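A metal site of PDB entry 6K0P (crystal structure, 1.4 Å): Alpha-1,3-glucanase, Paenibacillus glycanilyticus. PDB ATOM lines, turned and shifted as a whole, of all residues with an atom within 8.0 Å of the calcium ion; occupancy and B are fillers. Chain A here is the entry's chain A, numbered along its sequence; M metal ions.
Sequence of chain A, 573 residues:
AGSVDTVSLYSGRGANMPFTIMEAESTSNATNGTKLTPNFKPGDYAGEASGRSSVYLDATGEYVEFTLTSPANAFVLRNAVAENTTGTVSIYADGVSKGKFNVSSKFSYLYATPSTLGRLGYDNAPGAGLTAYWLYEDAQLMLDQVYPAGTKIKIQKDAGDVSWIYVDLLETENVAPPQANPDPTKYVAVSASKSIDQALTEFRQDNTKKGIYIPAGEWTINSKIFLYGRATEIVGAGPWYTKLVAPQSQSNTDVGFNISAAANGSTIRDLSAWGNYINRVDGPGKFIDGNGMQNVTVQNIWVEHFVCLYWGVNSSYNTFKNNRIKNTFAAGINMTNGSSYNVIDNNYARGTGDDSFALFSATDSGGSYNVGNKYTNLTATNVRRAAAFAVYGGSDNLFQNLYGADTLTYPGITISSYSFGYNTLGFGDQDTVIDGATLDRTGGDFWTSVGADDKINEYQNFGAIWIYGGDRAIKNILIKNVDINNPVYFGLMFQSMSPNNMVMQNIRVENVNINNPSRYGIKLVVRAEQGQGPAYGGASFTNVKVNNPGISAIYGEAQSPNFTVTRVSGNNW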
ATOM      1  N   ILE A  21       1.424   3.392  -5.116  1.00  0.00           N
ATOM      2  CA  ILE A  21       2.624   2.842  -4.479  1.00  0.00           C
ATOM      3  C   ILE A  21       2.207   1.743  -3.518  1.00  0.00           C
ATOM      4  O   ILE A  21       1.366   1.952  -2.639  1.00  0.00           O
ATOM      5  CB  ILE A  21       3.402   3.944  -3.732  1.00  0.00           C
ATOM      6  CG1 ILE A  21       3.916   4.971  -4.727  1.00  0.00           C
ATOM      7  CG2 ILE A  21       4.541   3.314  -2.914  1.00  0.00           C
ATOM      8  CD1 ILE A  21       4.436   6.211  -4.075  1.00  0.00           C
ATOM      9  N   MET A  22       2.802   0.567  -3.677  1.00  0.00           N
ATOM     10  CA  MET A  22       2.504  -0.567  -2.807  1.00  0.00           C
ATOM     11  C   MET A  22       3.776  -1.113  -2.207  1.00  0.00           C
ATOM     12  O   MET A  22       4.721  -1.449  -2.928  1.00  0.00           O
ATOM     13  CB  MET A  22       1.743  -1.642  -3.588  1.00  0.00           C
ATOM     14  CG  MET A  22       0.452  -1.096  -4.178  1.00  0.00           C
ATOM     15  SD  MET A  22      -0.689  -2.400  -4.645  1.00  0.00           S
ATOM     16  CE  MET A  22       0.244  -3.191  -5.914  1.00  0.00           C
ATOM     17  N   GLU A  23       3.820  -1.211  -0.880  1.00  0.00           N
ATOM     18  CA  GLU A  23       5.005  -1.718  -0.204  1.00  0.00           C
ATOM     19  C   GLU A  23       5.056  -3.237  -0.313  1.00  0.00           C
ATOM     20  O   GLU A  23       4.050  -3.924  -0.109  1.00  0.00           O
ATOM     21  CB  GLU A  23       4.988  -1.322   1.278  1.00  0.00           C
ATOM     22  CG  GLU A  23       5.021   0.179   1.527  1.00  0.00           C
ATOM     23  CD  GLU A  23       6.360   0.814   1.196  1.00  0.00           C
ATOM     24  OE1 GLU A  23       7.335   0.095   0.890  1.00  0.00           O
ATOM     25  OE2 GLU A  23       6.419   2.062   1.240  1.00  0.00           O
ATOM     26  N   ALA A  24       6.243  -3.759  -0.624  1.00  0.00           N
ATOM     27  CA  ALA A  24       6.395  -5.208  -0.782  1.00  0.00           C
ATOM     28  C   ALA A  24       6.053  -5.938   0.512  1.00  0.00           C
ATOM     29  O   ALA A  24       5.420  -7.005   0.476  1.00  0.00           O
ATOM     30  CB  ALA A  24       7.828  -5.536  -1.194  1.00  0.00           C
ATOM     31  N   GLU A  25       6.454  -5.371   1.647  1.00  0.00           N
ATOM     32  CA  GLU A  25       6.376  -6.010   2.958  1.00  0.00           C
ATOM     33  C   GLU A  25       4.988  -5.976   3.561  1.00  0.00           C
ATOM     34  O   GLU A  25       4.818  -6.448   4.700  1.00  0.00           O
ATOM     35  CB  GLU A  25       7.371  -5.351   3.923  1.00  0.00           C
ATOM     36  CG  GLU A  25       7.091  -3.876   4.220  1.00  0.00           C
ATOM     37  CD  GLU A  25       7.733  -2.908   3.217  1.00  0.00           C
ATOM     38  OE1 GLU A  25       8.101  -3.318   2.084  1.00  0.00           O
ATOM     39  OE2 GLU A  25       7.864  -1.717   3.573  1.00  0.00           O
ATOM     40  N   SER A  26       3.996  -5.437   2.856  1.00  0.00           N
ATOM     41  CA  SER A  26       2.655  -5.346   3.420  1.00  0.00           C
ATOM     42  C   SER A  26       2.174  -6.735   3.822  1.00  0.00           C
ATOM     43  O   SER A  26       2.438  -7.730   3.141  1.00  0.00           O
ATOM     44  CB  SER A  26       1.707  -4.765   2.383  1.00  0.00           C
ATOM     45  OG  SER A  26       0.348  -4.994   2.738  1.00  0.00           O
ATOM     46  N   TYR A  45      19.861  -2.197   4.249  1.00  0.00           N
ATOM     47  CA  TYR A  45      18.770  -2.509   3.312  1.00  0.00           C
ATOM     48  C   TYR A  45      17.382  -2.283   3.911  1.00  0.00           C
ATOM     49  O   TYR A  45      16.423  -2.073   3.158  1.00  0.00           O
ATOM     50  CB  TYR A  45      18.908  -3.919   2.731  1.00  0.00           C
ATOM     51  CG  TYR A  45      20.120  -4.046   1.833  1.00  0.00           C
ATOM     52  CD1 TYR A  45      20.161  -3.446   0.574  1.00  0.00           C
ATOM     53  CD2 TYR A  45      21.246  -4.737   2.269  1.00  0.00           C
ATOM     54  CE1 TYR A  45      21.298  -3.531  -0.218  1.00  0.00           C
ATOM     55  CE2 TYR A  45      22.386  -4.834   1.471  1.00  0.00           C
ATOM     56  CZ  TYR A  45      22.394  -4.238   0.228  1.00  0.00           C
ATOM     57  OH  TYR A  45      23.532  -4.338  -0.534  1.00  0.00           O
ATOM     58  N   ALA A  46      17.235  -2.354   5.242  1.00  0.00           N
ATOM     59  CA  ALA A  46      15.953  -1.970   5.839  1.00  0.00           C
ATOM     60  C   ALA A  46      15.896  -0.466   6.041  1.00  0.00           C
ATOM     61  O   ALA A  46      14.925   0.194   5.629  1.00  0.00           O
ATOM     62  CB  ALA A  46      15.752  -2.676   7.187  1.00  0.00           C
ATOM     63  N   GLU A  48      17.162   1.991   4.600  1.00  0.00           N
ATOM     64  CA  GLU A  48      17.039   2.802   3.385  1.00  0.00           C
ATOM     65  C   GLU A  48      15.802   2.493   2.564  1.00  0.00           C
ATOM     66  O   GLU A  48      15.579   3.141   1.540  1.00  0.00           O
ATOM     67  CB  GLU A  48      18.287   2.674   2.516  1.00  0.00           C
ATOM     68  CG  GLU A  48      19.540   3.272   3.158  1.00  0.00           C
ATOM     69  CD  GLU A  48      20.630   3.590   2.162  1.00  0.00           C
ATOM     70  OE1 GLU A  48      20.400   3.396   0.945  1.00  0.00           O
ATOM     71  OE2 GLU A  48      21.714   4.051   2.584  1.00  0.00           O
ATOM     72  N   ALA A  49      15.017   1.505   2.971  1.00  0.00           N
ATOM     73  CA  ALA A  49      13.823   1.127   2.219  1.00  0.00           C
ATOM     74  C   ALA A  49      12.651   2.043   2.556  1.00  0.00           C
ATOM     75  O   ALA A  49      12.560   2.610   3.654  1.00  0.00           O
ATOM     76  CB  ALA A  49      13.432  -0.316   2.562  1.00  0.00           C
ATOM     77  N   SER A  50      11.760   2.213   1.580  1.00  0.00           N
ATOM     78  CA  SER A  50      10.455   2.790   1.858  1.00  0.00           C
ATOM     79  C   SER A  50       9.743   1.959   2.920  1.00  0.00           C
ATOM     80  O   SER A  50       9.703   0.725   2.836  1.00  0.00           O
ATOM     81  CB  SER A  50       9.642   2.800   0.568  1.00  0.00           C
ATOM     82  OG  SER A  50       8.427   3.519   0.712  1.00  0.00           O
ATOM     83  N   GLY A  51       9.194   2.626   3.931  1.00  0.00           N
ATOM     84  CA  GLY A  51       8.599   1.907   5.039  1.00  0.00           C
ATOM     85  C   GLY A  51       9.608   1.258   5.955  1.00  0.00           C
ATOM     86  O   GLY A  51       9.216   0.529   6.864  1.00  0.00           O
ATOM     87  N   ARG A  52      10.904   1.507   5.738  1.00  0.00           N
ATOM     88  CA  ARG A  52      11.993   0.891   6.480  1.00  0.00           C
ATOM     89  C   ARG A  52      11.988  -0.629   6.389  1.00  0.00           C
ATOM     90  O   ARG A  52      12.511  -1.318   7.271  1.00  0.00           O
ATOM     91  CB  ARG A  52      12.082   1.374   7.942  1.00  0.00           C
ATOM     92  CG  ARG A  52      11.998   2.889   8.066  1.00  0.00           C
ATOM     93  CD  ARG A  52      13.200   3.600   7.416  1.00  0.00           C
ATOM     94  NE  ARG A  52      13.037   5.043   7.601  1.00  0.00           N
ATOM     95  CZ  ARG A  52      14.032   5.912   7.782  1.00  0.00           C
ATOM     96  NH1 ARG A  52      15.297   5.522   7.774  1.00  0.00           N
ATOM     97  NH2 ARG A  52      13.734   7.192   7.972  1.00  0.00           N
ATOM     98  N   SER A  53      11.416  -1.184   5.314  1.00  0.00           N
ATOM     99  CA  SER A  53      11.443  -2.622   5.131  1.00  0.00           C
ATOM    100  C   SER A  53      11.347  -2.968   3.646  1.00  0.00           C
ATOM    101  O   SER A  53      10.827  -2.214   2.826  1.00  0.00           O
ATOM    102  CB  SER A  53      10.325  -3.302   5.918  1.00  0.00           C
ATOM    103  OG  SER A  53      10.335  -4.716   5.731  1.00  0.00           O
ATOM    104  N   SER A  54      11.867  -4.155   3.328  1.00  0.00           N
ATOM    105  CA  SER A  54      11.763  -4.746   1.999  1.00  0.00           C
ATOM    106  C   SER A  54      11.601  -6.242   2.172  1.00  0.00           C
ATOM    107  O   SER A  54      11.726  -6.772   3.286  1.00  0.00           O
ATOM    108  CB  SER A  54      13.033  -4.498   1.178  1.00  0.00           C
ATOM    109  OG  SER A  54      13.165  -3.139   0.855  1.00  0.00           O
ATOM    110  N   VAL A  55      11.333  -6.933   1.069  1.00  0.00           N
ATOM    111  CA  VAL A  55      11.321  -8.395   1.068  1.00  0.00           C
ATOM    112  C   VAL A  55      12.503  -8.865   0.247  1.00  0.00           C
ATOM    113  O   VAL A  55      12.612  -8.541  -0.946  1.00  0.00           O
ATOM    114  CB  VAL A  55      10.001  -8.980   0.527  1.00  0.00           C
ATOM    115  CG1 VAL A  55      10.074 -10.498   0.552  1.00  0.00           C
ATOM    116  CG2 VAL A  55       8.820  -8.488   1.368  1.00  0.00           C
ATOM    117  N   PHE A  66       1.964  -9.068  -4.984  1.00  0.00           N
ATOM    118  CA  PHE A  66       1.162  -7.866  -4.823  1.00  0.00           C
ATOM    119  C   PHE A  66      -0.223  -8.108  -5.403  1.00  0.00           C
ATOM    120  O   PHE A  66      -0.435  -8.998  -6.232  1.00  0.00           O
ATOM    121  CB  PHE A  66       1.781  -6.696  -5.597  1.00  0.00           C
ATOM    122  CG  PHE A  66       3.138  -6.273  -5.119  1.00  0.00           C
ATOM    123  CD1 PHE A  66       4.282  -6.914  -5.555  1.00  0.00           C
ATOM    124  CD2 PHE A  66       3.282  -5.198  -4.249  1.00  0.00           C
ATOM    125  CE1 PHE A  66       5.538  -6.517  -5.132  1.00  0.00           C
ATOM    126  CE2 PHE A  66       4.531  -4.797  -3.820  1.00  0.00           C
ATOM    127  CZ  PHE A  66       5.660  -5.451  -4.265  1.00  0.00           C
ATOM    128  N   ARG A  78      11.136  -0.624  -7.105  1.00  0.00           N
ATOM    129  CA  ARG A  78      12.259  -0.131  -6.316  1.00  0.00           C
ATOM    130  C   ARG A  78      12.890  -1.319  -5.617  1.00  0.00           C
ATOM    131  O   ARG A  78      12.206  -2.083  -4.928  1.00  0.00           O
ATOM    132  CB  ARG A  78      11.843   0.926  -5.286  1.00  0.00           C
ATOM    133  CG  ARG A  78      13.039   1.618  -4.609  1.00  0.00           C
ATOM    134  CD  ARG A  78      12.592   2.764  -3.706  1.00  0.00           C
ATOM    135  NE  ARG A  78      13.663   3.735  -3.451  1.00  0.00           N
ATOM    136  CZ  ARG A  78      14.326   3.844  -2.297  1.00  0.00           C
ATOM    137  NH1 ARG A  78      14.081   3.023  -1.275  1.00  0.00           N
ATOM    138  NH2 ARG A  78      15.253   4.786  -2.169  1.00  0.00           N
ATOM    139  N   TYR A 136      19.292   1.560  -2.934  1.00  0.00           N
ATOM    140  CA  TYR A 136      18.132   1.236  -3.754  1.00  0.00           C
ATOM    141  C   TYR A 136      18.140   1.970  -5.084  1.00  0.00           C
ATOM    142  O   TYR A 136      18.699   3.062  -5.216  1.00  0.00           O
ATOM    143  CB  TYR A 136      16.830   1.537  -2.976  1.00  0.00           C
ATOM    144  CG  TYR A 136      16.560   0.458  -1.953  1.00  0.00           C
ATOM    145  CD1 TYR A 136      15.870  -0.693  -2.319  1.00  0.00           C
ATOM    146  CD2 TYR A 136      17.056   0.557  -0.665  1.00  0.00           C
ATOM    147  CE1 TYR A 136      15.665  -1.724  -1.407  1.00  0.00           C
ATOM    148  CE2 TYR A 136      16.845  -0.469   0.252  1.00  0.00           C
ATOM    149  CZ  TYR A 136      16.144  -1.600  -0.124  1.00  0.00           C
ATOM    150  OH  TYR A 136      15.926  -2.632   0.770  1.00  0.00           O
ATOM    151  N   VAL A 167      13.246  -6.374  -2.616  1.00  0.00           N
ATOM    152  CA  VAL A 167      12.105  -5.754  -3.268  1.00  0.00           C
ATOM    153  C   VAL A 167      11.450  -4.815  -2.256  1.00  0.00           C
ATOM    154  O   VAL A 167      10.936  -5.271  -1.227  1.00  0.00           O
ATOM    155  CB  VAL A 167      11.102  -6.798  -3.772  1.00  0.00           C
ATOM    156  CG1 VAL A 167       9.902  -6.106  -4.411  1.00  0.00           C
ATOM    157  CG2 VAL A 167      11.762  -7.743  -4.754  1.00  0.00           C
ATOM    158  N   ASP A 168      11.499  -3.513  -2.534  1.00  0.00           N
ATOM    159  CA  ASP A 168      11.069  -2.502  -1.577  1.00  0.00           C
ATOM    160  C   ASP A 168       9.606  -2.110  -1.788  1.00  0.00           C
ATOM    161  O   ASP A 168       8.804  -2.157  -0.844  1.00  0.00           O
ATOM    162  CB  ASP A 168      11.999  -1.281  -1.709  1.00  0.00           C
ATOM    163  CG  ASP A 168      11.659  -0.172  -0.746  1.00  0.00           C
ATOM    164  OD1 ASP A 168      10.814  -0.392   0.148  1.00  0.00           O
ATOM    165  OD2 ASP A 168      12.242   0.926  -0.852  1.00  0.00           O
ATOM    166  N   LEU A 169       9.267  -1.672  -2.995  1.00  0.00           N
ATOM    167  CA  LEU A 169       7.917  -1.251  -3.316  1.00  0.00           C
ATOM    168  C   LEU A 169       7.711  -1.441  -4.809  1.00  0.00           C
ATOM    169  O   LEU A 169       8.664  -1.612  -5.575  1.00  0.00           O
ATOM    170  CB  LEU A 169       7.651   0.219  -2.907  1.00  0.00           C
ATOM    171  CG  LEU A 169       8.471   1.334  -3.581  1.00  0.00           C
ATOM    172  CD1 LEU A 169       8.008   1.665  -5.009  1.00  0.00           C
ATOM    173  CD2 LEU A 169       8.445   2.607  -2.754  1.00  0.00           C
ATOM    174  N   LEU A 170       6.443  -1.366  -5.210  1.00  0.00           N
ATOM    175  CA  LEU A 170       6.036  -1.409  -6.607  1.00  0.00           C
ATOM    176  C   LEU A 170       5.124  -0.236  -6.884  1.00  0.00           C
ATOM    177  O   LEU A 170       4.143  -0.032  -6.162  1.00  0.00           O
ATOM    178  CB  LEU A 170       5.278  -2.726  -6.862  1.00  0.00           C
ATOM    179  CG  LEU A 170       4.828  -3.037  -8.288  1.00  0.00           C
ATOM    180  CD1 LEU A 170       6.045  -3.361  -9.138  1.00  0.00           C
ATOM    181  CD2 LEU A 170       3.830  -4.194  -8.273  1.00  0.00           C
ATOM    182  N   ASN A 382      11.782   8.862   0.765  1.00  0.00           N
ATOM    183  CA  ASN A 382      13.112   8.287   0.571  1.00  0.00           C
ATOM    184  C   ASN A 382      14.136   9.374   0.284  1.00  0.00           C
ATOM    185  O   ASN A 382      14.871   9.338  -0.719  1.00  0.00           O
ATOM    186  CB  ASN A 382      13.110   7.233  -0.547  1.00  0.00           C
ATOM    187  CG  ASN A 382      12.413   5.949  -0.143  1.00  0.00           C
ATOM    188  OD1 ASN A 382      11.461   5.526  -0.802  1.00  0.00           O
ATOM    189  ND2 ASN A 382      12.882   5.306   0.921  1.00  0.00           N
ATOM    190  N   ASP A 406      10.489   8.862   5.369  1.00  0.00           N
ATOM    191  CA  ASP A 406      11.689   8.045   5.228  1.00  0.00           C
ATOM    192  C   ASP A 406      12.902   8.876   4.804  1.00  0.00           C
ATOM    193  O   ASP A 406      13.507   8.665   3.750  1.00  0.00           O
ATOM    194  CB  ASP A 406      11.436   6.841   4.315  1.00  0.00           C
ATOM    195  CG  ASP A 406      10.457   5.868   4.929  1.00  0.00           C
ATOM    196  OD1 ASP A 406      10.631   5.574   6.140  1.00  0.00           O
ATOM    197  OD2 ASP A 406       9.526   5.411   4.232  1.00  0.00           O
ATOM    198  N   ARG A 441       8.093   8.628   9.729  1.00  0.00           N
ATOM    199  CA  ARG A 441       9.454   8.115   9.884  1.00  0.00           C
ATOM    200  C   ARG A 441      10.494   9.124   9.373  1.00  0.00           C
ATOM    201  O   ARG A 441      11.396   8.772   8.608  1.00  0.00           O
ATOM    202  CB  ARG A 441       9.627   6.735   9.236  1.00  0.00           C
ATOM    203  CG  ARG A 441       8.686   5.658   9.798  1.00  0.00           C
ATOM    204  CD  ARG A 441       8.702   4.344   8.971  1.00  0.00           C
ATOM    205  NE  ARG A 441       8.418   4.640   7.566  1.00  0.00           N
ATOM    206  CZ  ARG A 441       7.206   4.771   7.050  1.00  0.00           C
ATOM    207  NH1 ARG A 441       6.122   4.598   7.801  1.00  0.00           N
ATOM    208  NH2 ARG A 441       7.063   5.074   5.765  1.00  0.00           N
HETATM  209 CA    CA M   1       9.167  -1.162   1.509  1.00  0.00          CA
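The backbone carbonyl oxygen (O) of Asp 168 sits close to the backbone NH (N) of Ala 24. The side-chain carboxylate (OD2) of Asp 168 lies within salt-bridge range of the guanidinium group (NH1) of Arg 78, at 2.8 Å. N of Ser 50 lies close to ND2 of Asn 382 (3.4 Å).
The calcium ion is bound by OD1 of Asp 168 (2.3 Å), OE1 of Glu 23 (2.3 Å), O of Ser 53 (2.4 Å), O of Ser 50 (2.4 Å), OE1 of Glu 25 (2.5 Å), OE2 of Glu 25 (2.5 Å) and O of Asp 168 (2.6 Å). The calcium ion has seven donor atoms within binding distance.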
